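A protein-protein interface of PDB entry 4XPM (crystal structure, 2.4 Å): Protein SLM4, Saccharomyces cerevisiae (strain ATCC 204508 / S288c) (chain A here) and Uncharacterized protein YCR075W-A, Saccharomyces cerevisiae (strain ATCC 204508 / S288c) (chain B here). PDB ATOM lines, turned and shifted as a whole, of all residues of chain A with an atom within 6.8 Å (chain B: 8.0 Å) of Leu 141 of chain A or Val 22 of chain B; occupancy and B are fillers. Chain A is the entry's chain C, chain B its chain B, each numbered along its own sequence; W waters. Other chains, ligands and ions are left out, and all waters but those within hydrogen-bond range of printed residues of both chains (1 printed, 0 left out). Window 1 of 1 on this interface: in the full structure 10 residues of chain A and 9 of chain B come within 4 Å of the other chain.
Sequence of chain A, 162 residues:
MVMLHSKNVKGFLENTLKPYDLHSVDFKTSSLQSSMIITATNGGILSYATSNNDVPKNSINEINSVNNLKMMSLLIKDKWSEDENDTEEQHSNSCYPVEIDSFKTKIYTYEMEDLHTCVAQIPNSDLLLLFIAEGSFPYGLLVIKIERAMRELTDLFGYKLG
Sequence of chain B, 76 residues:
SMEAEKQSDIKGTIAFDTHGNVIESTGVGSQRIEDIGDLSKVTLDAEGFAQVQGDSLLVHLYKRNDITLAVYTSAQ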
ATOM      1  N   TYR A  20       3.540 -33.094 -17.337  1.00  0.00           N
ATOM      2  CA  TYR A  20       4.399 -31.919 -17.347  1.00  0.00           C
ATOM      3  C   TYR A  20       4.322 -31.267 -15.970  1.00  0.00           C
ATOM      4  O   TYR A  20       3.272 -31.296 -15.318  1.00  0.00           O
ATOM      5  CB  TYR A  20       3.937 -30.920 -18.405  1.00  0.00           C
ATOM      6  CG  TYR A  20       4.219 -31.354 -19.815  1.00  0.00           C
ATOM      7  CD1 TYR A  20       5.455 -31.121 -20.393  1.00  0.00           C
ATOM      8  CD2 TYR A  20       3.252 -31.994 -20.565  1.00  0.00           C
ATOM      9  CE1 TYR A  20       5.719 -31.509 -21.677  1.00  0.00           C
ATOM     10  CE2 TYR A  20       3.504 -32.386 -21.846  1.00  0.00           C
ATOM     11  CZ  TYR A  20       4.739 -32.142 -22.403  1.00  0.00           C
ATOM     12  OH  TYR A  20       4.987 -32.531 -23.699  1.00  0.00           O
ATOM     13  N   LEU A  22       5.754 -27.661 -14.501  1.00  0.00           N
ATOM     14  CA  LEU A  22       6.508 -26.448 -14.768  1.00  0.00           C
ATOM     15  C   LEU A  22       6.762 -25.706 -13.465  1.00  0.00           C
ATOM     16  O   LEU A  22       5.985 -25.810 -12.514  1.00  0.00           O
ATOM     17  CB  LEU A  22       5.746 -25.569 -15.760  1.00  0.00           C
ATOM     18  CG  LEU A  22       5.930 -25.859 -17.260  1.00  0.00           C
ATOM     19  CD1 LEU A  22       6.002 -27.333 -17.587  1.00  0.00           C
ATOM     20  CD2 LEU A  22       4.825 -25.211 -18.080  1.00  0.00           C
ATOM     21  N   PHE A  27       2.349 -24.476 -13.021  1.00  0.00           N
ATOM     22  CA  PHE A  27       1.498 -25.297 -13.871  1.00  0.00           C
ATOM     23  C   PHE A  27       1.950 -26.743 -13.940  1.00  0.00           C
ATOM     24  O   PHE A  27       3.133 -27.039 -14.072  1.00  0.00           O
ATOM     25  CB  PHE A  27       1.405 -24.711 -15.286  1.00  0.00           C
ATOM     26  CG  PHE A  27       0.608 -25.560 -16.248  1.00  0.00           C
ATOM     27  CD1 PHE A  27      -0.772 -25.418 -16.337  1.00  0.00           C
ATOM     28  CD2 PHE A  27       1.239 -26.494 -17.068  1.00  0.00           C
ATOM     29  CE1 PHE A  27      -1.505 -26.188 -17.227  1.00  0.00           C
ATOM     30  CE2 PHE A  27       0.516 -27.263 -17.960  1.00  0.00           C
ATOM     31  CZ  PHE A  27      -0.858 -27.113 -18.045  1.00  0.00           C
ATOM     32  N   LYS A  28       0.980 -27.637 -13.897  1.00  0.00           N
ATOM     33  CA  LYS A  28       1.258 -29.060 -13.847  1.00  0.00           C
ATOM     34  C   LYS A  28       0.060 -29.795 -14.421  1.00  0.00           C
ATOM     35  O   LYS A  28      -1.084 -29.436 -14.138  1.00  0.00           O
ATOM     36  CB  LYS A  28       1.488 -29.470 -12.398  1.00  0.00           C
ATOM     37  CG  LYS A  28       1.400 -30.951 -12.126  1.00  0.00           C
ATOM     38  CD  LYS A  28       1.298 -31.218 -10.626  1.00  0.00           C
ATOM     39  CE  LYS A  28       0.138 -30.434  -9.998  1.00  0.00           C
ATOM     40  NZ  LYS A  28      -1.182 -30.727 -10.644  1.00  0.00           N
ATOM     41  N   THR A  29       0.314 -30.802 -15.247  1.00  0.00           N
ATOM     42  CA  THR A  29      -0.769 -31.643 -15.744  1.00  0.00           C
ATOM     43  C   THR A  29      -0.826 -32.890 -14.906  1.00  0.00           C
ATOM     44  O   THR A  29       0.108 -33.190 -14.160  1.00  0.00           O
ATOM     45  CB  THR A  29      -0.556 -32.073 -17.204  1.00  0.00           C
ATOM     46  OG1 THR A  29       0.515 -33.029 -17.283  1.00  0.00           O
ATOM     47  CG2 THR A  29      -0.241 -30.860 -18.074  1.00  0.00           C
ATOM     48  N   TYR A  96      -2.545 -30.847 -37.356  1.00  0.00           N
ATOM     49  CA  TYR A  96      -1.218 -30.210 -37.385  1.00  0.00           C
ATOM     50  C   TYR A  96      -0.285 -30.969 -38.320  1.00  0.00           C
ATOM     51  O   TYR A  96       0.195 -32.047 -37.979  1.00  0.00           O
ATOM     52  CB  TYR A  96      -0.564 -30.183 -35.997  1.00  0.00           C
ATOM     53  CG  TYR A  96      -1.250 -29.368 -34.917  1.00  0.00           C
ATOM     54  CD1 TYR A  96      -2.425 -29.812 -34.312  1.00  0.00           C
ATOM     55  CD2 TYR A  96      -0.691 -28.174 -34.465  1.00  0.00           C
ATOM     56  CE1 TYR A  96      -3.034 -29.065 -33.302  1.00  0.00           C
ATOM     57  CE2 TYR A  96      -1.284 -27.433 -33.468  1.00  0.00           C
ATOM     58  CZ  TYR A  96      -2.450 -27.874 -32.886  1.00  0.00           C
ATOM     59  OH  TYR A  96      -3.026 -27.123 -31.887  1.00  0.00           O
ATOM     60  N   CYS A 118      -5.006 -37.215 -28.811  1.00  0.00           N
ATOM     61  CA  CYS A 118      -4.233 -36.887 -29.991  1.00  0.00           C
ATOM     62  C   CYS A 118      -3.878 -38.177 -30.661  1.00  0.00           C
ATOM     63  O   CYS A 118      -3.574 -39.163 -29.995  1.00  0.00           O
ATOM     64  CB  CYS A 118      -2.940 -36.166 -29.626  1.00  0.00           C
ATOM     65  SG  CYS A 118      -3.156 -34.451 -29.552  1.00  0.00           S
ATOM     66  N   PHE A 137      -6.144 -31.641 -19.592  1.00  0.00           N
ATOM     67  CA  PHE A 137      -4.849 -31.609 -20.260  1.00  0.00           C
ATOM     68  C   PHE A 137      -4.981 -30.768 -21.529  1.00  0.00           C
ATOM     69  O   PHE A 137      -5.706 -31.154 -22.444  1.00  0.00           O
ATOM     70  CB  PHE A 137      -4.419 -33.036 -20.612  1.00  0.00           C
ATOM     71  CG  PHE A 137      -2.930 -33.203 -20.812  1.00  0.00           C
ATOM     72  CD1 PHE A 137      -2.282 -32.611 -21.887  1.00  0.00           C
ATOM     73  CD2 PHE A 137      -2.184 -33.973 -19.934  1.00  0.00           C
ATOM     74  CE1 PHE A 137      -0.921 -32.769 -22.072  1.00  0.00           C
ATOM     75  CE2 PHE A 137      -0.816 -34.145 -20.123  1.00  0.00           C
ATOM     76  CZ  PHE A 137      -0.187 -33.543 -21.190  1.00  0.00           C
ATOM     77  N   PRO A 138      -4.287 -29.615 -21.585  1.00  0.00           N
ATOM     78  CA  PRO A 138      -4.452 -28.673 -22.713  1.00  0.00           C
ATOM     79  C   PRO A 138      -4.056 -29.311 -24.039  1.00  0.00           C
ATOM     80  O   PRO A 138      -3.008 -29.958 -24.112  1.00  0.00           O
ATOM     81  CB  PRO A 138      -3.499 -27.513 -22.370  1.00  0.00           C
ATOM     82  CG  PRO A 138      -3.212 -27.665 -20.879  1.00  0.00           C
ATOM     83  CD  PRO A 138      -3.282 -29.153 -20.610  1.00  0.00           C
ATOM     84  N   TYR A 139      -4.903 -29.152 -25.053  1.00  0.00           N
ATOM     85  CA  TYR A 139      -4.701 -29.771 -26.365  1.00  0.00           C
ATOM     86  C   TYR A 139      -3.371 -29.376 -27.005  1.00  0.00           C
ATOM     87  O   TYR A 139      -2.635 -30.241 -27.502  1.00  0.00           O
ATOM     88  CB  TYR A 139      -5.850 -29.409 -27.314  1.00  0.00           C
ATOM     89  CG  TYR A 139      -7.036 -30.353 -27.243  1.00  0.00           C
ATOM     90  CD1 TYR A 139      -6.905 -31.686 -27.636  1.00  0.00           C
ATOM     91  CD2 TYR A 139      -8.290 -29.913 -26.793  1.00  0.00           C
ATOM     92  CE1 TYR A 139      -7.977 -32.563 -27.587  1.00  0.00           C
ATOM     93  CE2 TYR A 139      -9.380 -30.787 -26.737  1.00  0.00           C
ATOM     94  CZ  TYR A 139      -9.208 -32.114 -27.143  1.00  0.00           C
ATOM     95  OH  TYR A 139     -10.253 -33.009 -27.110  1.00  0.00           O
ATOM     96  N   GLY A 140      -3.066 -28.075 -26.992  1.00  0.00           N
ATOM     97  CA  GLY A 140      -1.800 -27.586 -27.516  1.00  0.00           C
ATOM     98  C   GLY A 140      -0.608 -28.289 -26.876  1.00  0.00           C
ATOM     99  O   GLY A 140       0.366 -28.626 -27.552  1.00  0.00           O
ATOM    100  N   LEU A 141      -0.691 -28.533 -25.573  1.00  0.00           N
ATOM    101  CA  LEU A 141       0.363 -29.255 -24.876  1.00  0.00           C
ATOM    102  C   LEU A 141       0.388 -30.729 -25.286  1.00  0.00           C
ATOM    103  O   LEU A 141       1.473 -31.311 -25.476  1.00  0.00           O
ATOM    104  CB  LEU A 141       0.205 -29.097 -23.362  1.00  0.00           C
ATOM    105  CG  LEU A 141       1.356 -29.592 -22.469  1.00  0.00           C
ATOM    106  CD1 LEU A 141       2.688 -28.975 -22.855  1.00  0.00           C
ATOM    107  CD2 LEU A 141       1.051 -29.260 -21.027  1.00  0.00           C
ATOM    108  N   LEU A 142      -0.800 -31.325 -25.439  1.00  0.00           N
ATOM    109  CA  LEU A 142      -0.917 -32.723 -25.853  1.00  0.00           C
ATOM    110  C   LEU A 142      -0.252 -32.934 -27.217  1.00  0.00           C
ATOM    111  O   LEU A 142       0.457 -33.921 -27.460  1.00  0.00           O
ATOM    112  CB  LEU A 142      -2.394 -33.104 -25.970  1.00  0.00           C
ATOM    113  CG  LEU A 142      -2.896 -34.392 -25.320  1.00  0.00           C
ATOM    114  CD1 LEU A 142      -4.098 -34.953 -26.064  1.00  0.00           C
ATOM    115  CD2 LEU A 142      -1.806 -35.414 -25.207  1.00  0.00           C
ATOM    116  N   VAL A 143      -0.503 -31.992 -28.112  1.00  0.00           N
ATOM    117  CA  VAL A 143       0.036 -32.049 -29.464  1.00  0.00           C
ATOM    118  C   VAL A 143       1.570 -32.008 -29.456  1.00  0.00           C
ATOM    119  O   VAL A 143       2.224 -32.789 -30.163  1.00  0.00           O
ATOM    120  CB  VAL A 143      -0.581 -30.917 -30.335  1.00  0.00           C
ATOM    121  CG1 VAL A 143       0.250 -30.658 -31.580  1.00  0.00           C
ATOM    122  CG2 VAL A 143      -2.018 -31.295 -30.696  1.00  0.00           C
ATOM    123  N   ILE A 144       2.137 -31.110 -28.646  1.00  0.00           N
ATOM    124  CA  ILE A 144       3.587 -31.025 -28.475  1.00  0.00           C
ATOM    125  C   ILE A 144       4.143 -32.342 -27.922  1.00  0.00           C
ATOM    126  O   ILE A 144       5.135 -32.868 -28.441  1.00  0.00           O
ATOM    127  CB  ILE A 144       3.994 -29.833 -27.584  1.00  0.00           C
ATOM    128  CG1 ILE A 144       3.763 -28.511 -28.333  1.00  0.00           C
ATOM    129  CG2 ILE A 144       5.467 -29.941 -27.164  1.00  0.00           C
ATOM    130  CD1 ILE A 144       3.772 -27.240 -27.426  1.00  0.00           C
ATOM    131  N   LYS A 145       3.481 -32.886 -26.902  1.00  0.00           N
ATOM    132  CA  LYS A 145       3.892 -34.159 -26.297  1.00  0.00           C
ATOM    133  C   LYS A 145       3.974 -35.272 -27.354  1.00  0.00           C
ATOM    134  O   LYS A 145       4.966 -36.000 -27.437  1.00  0.00           O
ATOM    135  CB  LYS A 145       2.918 -34.556 -25.176  1.00  0.00           C
ATOM    136  CG  LYS A 145       3.491 -35.523 -24.133  1.00  0.00           C
ATOM    137  CD  LYS A 145       2.393 -35.976 -23.151  1.00  0.00           C
ATOM    138  CE  LYS A 145       2.927 -36.172 -21.730  1.00  0.00           C
ATOM    139  NZ  LYS A 145       4.213 -36.950 -21.650  1.00  0.00           N
ATOM    140  N   ILE A 146       2.942 -35.386 -28.182  1.00  0.00           N
ATOM    141  CA  ILE A 146       2.907 -36.465 -29.176  1.00  0.00           C
ATOM    142  C   ILE A 146       3.900 -36.225 -30.309  1.00  0.00           C
ATOM    143  O   ILE A 146       4.503 -37.163 -30.803  1.00  0.00           O
ATOM    144  CB  ILE A 146       1.460 -36.737 -29.707  1.00  0.00           C
ATOM    145  CG1 ILE A 146       1.337 -38.157 -30.266  1.00  0.00           C
ATOM    146  CG2 ILE A 146       1.024 -35.700 -30.733  1.00  0.00           C
ATOM    147  CD1 ILE A 146      -0.094 -38.556 -30.552  1.00  0.00           C
ATOM    148  N   THR B  13      -1.536 -16.323 -16.435  1.00  0.00           N
ATOM    149  CA  THR B  13      -0.922 -16.501 -17.751  1.00  0.00           C
ATOM    150  C   THR B  13      -1.765 -17.458 -18.579  1.00  0.00           C
ATOM    151  O   THR B  13      -2.498 -18.294 -18.032  1.00  0.00           O
ATOM    152  CB  THR B  13       0.500 -17.127 -17.671  1.00  0.00           C
ATOM    153  OG1 THR B  13       0.381 -18.537 -17.439  1.00  0.00           O
ATOM    154  CG2 THR B  13       1.352 -16.501 -16.539  1.00  0.00           C
ATOM    155  N   ILE B  14      -1.666 -17.313 -19.897  1.00  0.00           N
ATOM    156  CA  ILE B  14      -2.127 -18.315 -20.849  1.00  0.00           C
ATOM    157  C   ILE B  14      -1.072 -18.406 -21.941  1.00  0.00           C
ATOM    158  O   ILE B  14      -0.650 -17.382 -22.478  1.00  0.00           O
ATOM    159  CB  ILE B  14      -3.430 -17.914 -21.578  1.00  0.00           C
ATOM    160  CG1 ILE B  14      -4.532 -17.516 -20.604  1.00  0.00           C
ATOM    161  CG2 ILE B  14      -3.902 -19.050 -22.504  1.00  0.00           C
ATOM    162  CD1 ILE B  14      -5.852 -17.132 -21.318  1.00  0.00           C
ATOM    163  N   ALA B  15      -0.643 -19.615 -22.275  1.00  0.00           N
ATOM    164  CA  ALA B  15       0.123 -19.803 -23.498  1.00  0.00           C
ATOM    165  C   ALA B  15      -0.750 -20.568 -24.471  1.00  0.00           C
ATOM    166  O   ALA B  15      -1.459 -21.495 -24.074  1.00  0.00           O
ATOM    167  CB  ALA B  15       1.405 -20.567 -23.224  1.00  0.00           C
ATOM    168  N   PHE B  16      -0.702 -20.182 -25.746  1.00  0.00           N
ATOM    169  CA  PHE B  16      -1.468 -20.878 -26.764  1.00  0.00           C
ATOM    170  C   PHE B  16      -0.760 -20.915 -28.107  1.00  0.00           C
ATOM    171  O   PHE B  16       0.114 -20.092 -28.366  1.00  0.00           O
ATOM    172  CB  PHE B  16      -2.856 -20.256 -26.910  1.00  0.00           C
ATOM    173  CG  PHE B  16      -2.852 -18.811 -27.329  1.00  0.00           C
ATOM    174  CD1 PHE B  16      -2.867 -18.466 -28.675  1.00  0.00           C
ATOM    175  CD2 PHE B  16      -2.879 -17.798 -26.376  1.00  0.00           C
ATOM    176  CE1 PHE B  16      -2.904 -17.123 -29.075  1.00  0.00           C
ATOM    177  CE2 PHE B  16      -2.910 -16.458 -26.755  1.00  0.00           C
ATOM    178  CZ  PHE B  16      -2.923 -16.115 -28.112  1.00  0.00           C
ATOM    179  N   ASP B  17      -1.151 -21.860 -28.964  1.00  0.00           N
ATOM    180  CA  ASP B  17      -0.457 -22.066 -30.222  1.00  0.00           C
ATOM    181  C   ASP B  17      -1.198 -21.370 -31.367  1.00  0.00           C
ATOM    182  O   ASP B  17      -2.193 -20.681 -31.127  1.00  0.00           O
ATOM    183  CB  ASP B  17      -0.227 -23.573 -30.489  1.00  0.00           C
ATOM    184  CG  ASP B  17      -1.537 -24.368 -30.735  1.00  0.00           C
ATOM    185  OD1 ASP B  17      -2.586 -23.779 -31.101  1.00  0.00           O
ATOM    186  OD2 ASP B  17      -1.502 -25.612 -30.594  1.00  0.00           O
ATOM    187  N   HIS B  19      -3.097 -22.565 -33.736  1.00  0.00           N
ATOM    188  CA  HIS B  19      -4.469 -23.025 -33.919  1.00  0.00           C
ATOM    189  C   HIS B  19      -5.378 -22.405 -32.836  1.00  0.00           C
ATOM    190  O   HIS B  19      -6.585 -22.604 -32.847  1.00  0.00           O
ATOM    191  CB  HIS B  19      -4.565 -24.556 -33.820  1.00  0.00           C
ATOM    192  CG  HIS B  19      -3.929 -25.302 -34.958  1.00  0.00           C
ATOM    193  ND1 HIS B  19      -2.651 -25.041 -35.407  1.00  0.00           N
ATOM    194  CD2 HIS B  19      -4.388 -26.334 -35.713  1.00  0.00           C
ATOM    195  CE1 HIS B  19      -2.360 -25.858 -36.409  1.00  0.00           C
ATOM    196  NE2 HIS B  19      -3.394 -26.657 -36.608  1.00  0.00           N
ATOM    197  N   GLY B  20      -4.803 -21.670 -31.890  1.00  0.00           N
ATOM    198  CA  GLY B  20      -5.586 -21.142 -30.785  1.00  0.00           C
ATOM    199  C   GLY B  20      -5.790 -22.145 -29.645  1.00  0.00           C
ATOM    200  O   GLY B  20      -6.601 -21.904 -28.748  1.00  0.00           O
ATOM    201  N   ASN B  21      -5.071 -23.270 -29.664  1.00  0.00           N
ATOM    202  CA  ASN B  21      -5.212 -24.270 -28.598  1.00  0.00           C
ATOM    203  C   ASN B  21      -4.320 -23.952 -27.410  1.00  0.00           C
ATOM    204  O   ASN B  21      -3.225 -23.405 -27.574  1.00  0.00           O
ATOM    205  CB  ASN B  21      -4.941 -25.679 -29.117  1.00  0.00           C
ATOM    206  CG  ASN B  21      -6.126 -26.244 -29.889  1.00  0.00           C
ATOM    207  OD1 ASN B  21      -7.273 -26.031 -29.509  1.00  0.00           O
ATOM    208  ND2 ASN B  21      -5.852 -26.950 -30.978  1.00  0.00           N
ATOM    209  N   VAL B  22      -4.773 -24.264 -26.208  1.00  0.00           N
ATOM    210  CA  VAL B  22      -3.969 -23.859 -25.065  1.00  0.00           C
ATOM    211  C   VAL B  22      -2.852 -24.842 -24.812  1.00  0.00           C
ATOM    212  O   VAL B  22      -2.988 -26.042 -25.048  1.00  0.00           O
ATOM    213  CB  VAL B  22      -4.804 -23.444 -23.795  1.00  0.00           C
ATOM    214  CG1 VAL B  22      -6.283 -23.766 -23.958  1.00  0.00           C
ATOM    215  CG2 VAL B  22      -4.224 -24.013 -22.515  1.00  0.00           C
ATOM    216  N   ILE B  23      -1.713 -24.288 -24.423  1.00  0.00           N
ATOM    217  CA  ILE B  23      -0.550 -25.053 -24.009  1.00  0.00           C
ATOM    218  C   ILE B  23      -0.427 -25.064 -22.475  1.00  0.00           C
ATOM    219  O   ILE B  23       0.008 -26.057 -21.866  1.00  0.00           O
ATOM    220  CB  ILE B  23       0.703 -24.453 -24.651  1.00  0.00           C
ATOM    221  CG1 ILE B  23       0.675 -24.706 -26.164  1.00  0.00           C
ATOM    222  CG2 ILE B  23       1.932 -25.030 -24.043  1.00  0.00           C
ATOM    223  CD1 ILE B  23       1.254 -23.594 -26.985  1.00  0.00           C
ATOM    224  N   GLU B  24      -0.823 -23.960 -21.851  1.00  0.00           N
ATOM    225  CA  GLU B  24      -0.902 -23.903 -20.388  1.00  0.00           C
ATOM    226  C   GLU B  24      -1.679 -22.674 -19.964  1.00  0.00           C
ATOM    227  O   GLU B  24      -1.818 -21.713 -20.738  1.00  0.00           O
ATOM    228  CB  GLU B  24       0.484 -23.906 -19.728  1.00  0.00           C
ATOM    229  CG  GLU B  24       1.323 -22.615 -19.926  1.00  0.00           C
ATOM    230  CD  GLU B  24       0.988 -21.483 -18.928  1.00  0.00           C
ATOM    231  OE1 GLU B  24       1.120 -20.304 -19.310  1.00  0.00           O
ATOM    232  OE2 GLU B  24       0.600 -21.764 -17.770  1.00  0.00           O
ATOM    233  N   SER B  25      -2.174 -22.707 -18.732  1.00  0.00           N
ATOM    234  CA  SER B  25      -2.846 -21.544 -18.159  1.00  0.00           C
ATOM    235  C   SER B  25      -2.796 -21.609 -16.640  1.00  0.00           C
ATOM    236  O   SER B  25      -2.814 -22.692 -16.056  1.00  0.00           O
ATOM    237  CB  SER B  25      -4.295 -21.420 -18.666  1.00  0.00           C
ATOM    238  OG  SER B  25      -5.134 -22.367 -18.028  1.00  0.00           O
ATOM    239  N   THR B  26      -2.702 -20.435 -16.020  1.00  0.00           N
ATOM    240  CA  THR B  26      -2.578 -20.274 -14.572  1.00  0.00           C
ATOM    241  C   THR B  26      -3.315 -18.998 -14.183  1.00  0.00           C
ATOM    242  O   THR B  26      -3.616 -18.156 -15.051  1.00  0.00           O
ATOM    243  CB  THR B  26      -1.117 -20.061 -14.153  1.00  0.00           C
ATOM    244  OG1 THR B  26      -0.547 -19.028 -14.976  1.00  0.00           O
ATOM    245  CG2 THR B  26      -0.295 -21.345 -14.303  1.00  0.00           C
ATOM    246  N   GLY B  29      -5.828 -16.619 -15.902  1.00  0.00           N
ATOM    247  CA  GLY B  29      -5.678 -17.153 -17.239  1.00  0.00           C
ATOM    248  C   GLY B  29      -6.610 -18.324 -17.466  1.00  0.00           C
ATOM    249  O   GLY B  29      -7.252 -18.413 -18.514  1.00  0.00           O
ATOM    250  N   SER B  30      -6.701 -19.210 -16.470  1.00  0.00           N
ATOM    251  CA  SER B  30      -7.569 -20.388 -16.558  1.00  0.00           C
ATOM    252  C   SER B  30      -9.060 -20.029 -16.584  1.00  0.00           C
ATOM    253  O   SER B  30      -9.889 -20.817 -17.042  1.00  0.00           O
ATOM    254  CB  SER B  30      -7.285 -21.345 -15.402  1.00  0.00           C
ATOM    255  OG  SER B  30      -5.922 -21.737 -15.402  1.00  0.00           O
ATOM    256  N   ILE B  33      -9.878 -18.367 -20.591  1.00  0.00           N
ATOM    257  CA  ILE B  33      -9.527 -19.106 -21.798  1.00  0.00           C
ATOM    258  C   ILE B  33     -10.258 -18.576 -23.033  1.00  0.00           C
ATOM    259  O   ILE B  33      -9.706 -18.564 -24.133  1.00  0.00           O
ATOM    260  CB  ILE B  33      -9.810 -20.607 -21.612  1.00  0.00           C
ATOM    261  CG1 ILE B  33      -8.923 -21.163 -20.505  1.00  0.00           C
ATOM    262  CG2 ILE B  33      -9.531 -21.389 -22.881  1.00  0.00           C
ATOM    263  CD1 ILE B  33      -7.452 -21.136 -20.851  1.00  0.00           C
ATOM    264  N   GLU B  34     -11.480 -18.092 -22.858  1.00  0.00           N
ATOM    265  CA  GLU B  34     -12.236 -17.590 -24.005  1.00  0.00           C
ATOM    266  C   GLU B  34     -11.592 -16.361 -24.656  1.00  0.00           C
ATOM    267  O   GLU B  34     -11.911 -16.038 -25.795  1.00  0.00           O
ATOM    268  CB  GLU B  34     -13.691 -17.303 -23.632  1.00  0.00           C
ATOM    269  CG  GLU B  34     -14.435 -18.503 -23.066  1.00  0.00           C
ATOM    270  CD  GLU B  34     -14.463 -18.507 -21.545  1.00  0.00           C
ATOM    271  OE1 GLU B  34     -15.565 -18.352 -20.974  1.00  0.00           O
ATOM    272  OE2 GLU B  34     -13.388 -18.656 -20.925  1.00  0.00           O
ATOM    273  N   ILE B  36      -8.800 -16.092 -25.894  1.00  0.00           N
ATOM    274  CA  ILE B  36      -7.824 -16.480 -26.912  1.00  0.00           C
ATOM    275  C   ILE B  36      -8.271 -16.068 -28.300  1.00  0.00           C
ATOM    276  O   ILE B  36      -7.467 -15.605 -29.099  1.00  0.00           O
ATOM    277  CB  ILE B  36      -7.515 -17.990 -26.879  1.00  0.00           C
ATOM    278  CG1 ILE B  36      -6.693 -18.330 -25.635  1.00  0.00           C
ATOM    279  CG2 ILE B  36      -6.748 -18.409 -28.119  1.00  0.00           C
ATOM    280  CD1 ILE B  36      -6.520 -19.805 -25.396  1.00  0.00           C
ATOM    281  N   THR B  68       2.225 -18.073 -28.418  1.00  0.00           N
ATOM    282  CA  THR B  68       1.948 -16.780 -27.852  1.00  0.00           C
ATOM    283  C   THR B  68       1.837 -16.910 -26.351  1.00  0.00           C
ATOM    284  O   THR B  68       1.153 -17.803 -25.868  1.00  0.00           O
ATOM    285  CB  THR B  68       0.630 -16.207 -28.384  1.00  0.00           C
ATOM    286  OG1 THR B  68       0.689 -16.119 -29.810  1.00  0.00           O
ATOM    287  CG2 THR B  68       0.392 -14.829 -27.791  1.00  0.00           C
HETATM  288  O   HOH W   1       0.874 -26.777 -29.806  1.00  0.00           O
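The backbone carbonyl oxygen (O) of Val 22 of chain B is in hydrogen-bond range of the backbone NH (N) of Leu 141 of chain A, at 3.4 Å. The backbone carbonyl oxygen of Val 22 of chain B lies within hydrogen-bond range of the backbone NH of Gly 140 of chain A, 2.8 Å away. The side-chain carboxylate of Asp 17 of chain B sits at hydrogen-bond distance from the side-chain hydroxyl of Tyr 96 of chain A. ND2 of Asn 21 of chain B sits at hydrogen-bond distance from OH of Tyr 96 of chain A.
O of Phe 27 of chain A is in hydrogen-bond range of N of Leu 22 of chain A. The backbone NH (N) of Asn 21 of chain B sits at hydrogen-bond distance from the side-chain carboxylate (OD1) of Asp 17 of chain B, 2.9 Å away. The side-chain hydroxyl of Ser 25 of chain B is in hydrogen-bond range of the side-chain hydroxyl of Ser 30 of chain B (2.8 Å). OG1 of Thr 13 of chain B lies within hydrogen-bond range of OG1 of Thr 26 of chain B, 2.7 Å away. OD1 of Asp 17 of chain B lies within hydrogen-bond range of N of His 19 of chain B (2.9 Å). The backbone carbonyl oxygen (O) of Ala 15 of chain B lies within hydrogen-bond range of the backbone NH (N) of Ile 23 of chain B (2.8 Å).
Among the printed residues, merely in contact across the chains: Pro 138 of chain A with Val 22 of chain B (3.1 Å), Tyr 96 of chain A with His 19 of chain B (3.4 Å), Leu 141 of chain A with Ile 23 of chain B (3.4 Å), Phe 27 of chain A with Ser 25 of chain B (3.4 Å), Tyr 139 of chain A with Val 22 of chain B (3.7 Å), Gly 140 of chain A with Asp 17 of chain B (3.7 Å), Gly 140 of chain A with Asn 21 of chain B (3.7 Å), Pro 138 of chain A with Ile 23 of chain B (3.7 Å), Phe 27 of chain A with Glu 24 of chain B (3.8 Å), Gly 140 of chain A with Ile 23 of chain B (3.9 Å) and Phe 27 of chain A with Thr 26 of chain B (3.9 Å).
Leu 141 of chain A touches just these residues of chain B: Val 22 and Ile 23. Of the printed residues of chain A, Val 22 of chain B touches Pro 138 (3.1 Å), Tyr 139 (3.7 Å), Gly 140 (2.8 Å) and Leu 141 (3.4 Å). Of chain B, only Asp 17, Asn 21, Val 22 and Ile 23 come within 4 Å of Gly 140 of chain A. Of the printed residues of chain A, His 19 of chain B touches Tyr 96 (3.4 Å). Of the printed residues of chain B, Pro 138 of chain A touches Val 22 and Ile 23. Printed residues of chain A within 4 Å of Asp 17 of chain B: Tyr 96 and Gly 140. Of the printed residues of chain A, Ser 25 of chain B touches Phe 27. Thr 13 of chain B touches none of the printed residues of chain A. The nearest residue of chain B that does not touch Leu 141 of chain A is Glu 24 of chain B (5.5 Å). The nearest residue of chain A that does not touch Val 22 of chain B is Leu 142 of chain A (5.7 Å).
Along chain A the printed residues that touch a printed residue of chain B span positions 27 to 141. Printed residues of chain B that touch a printed residue of chain A: Asp 17, His 19, Asn 21, Val 22, Ile 23, Glu 24, Ser 25 and Thr 26. Hydrophobic or aromatic side chains of chain B within 4 Å of the printed part of chain A: His 19, Val 22 and Ile 23. Among the printed residues, 15 pairs touch across the chains. Among the printed residues, no Asp or Glu carboxylate lies within 4 Å of a Lys or Arg side-chain nitrogen of the other chain.
Water W1 lies within hydrogen-bond range of OD2 of Asp 17 of chain B (2.8 Å) and O of Gly 140 of chain A (3.0 Å).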
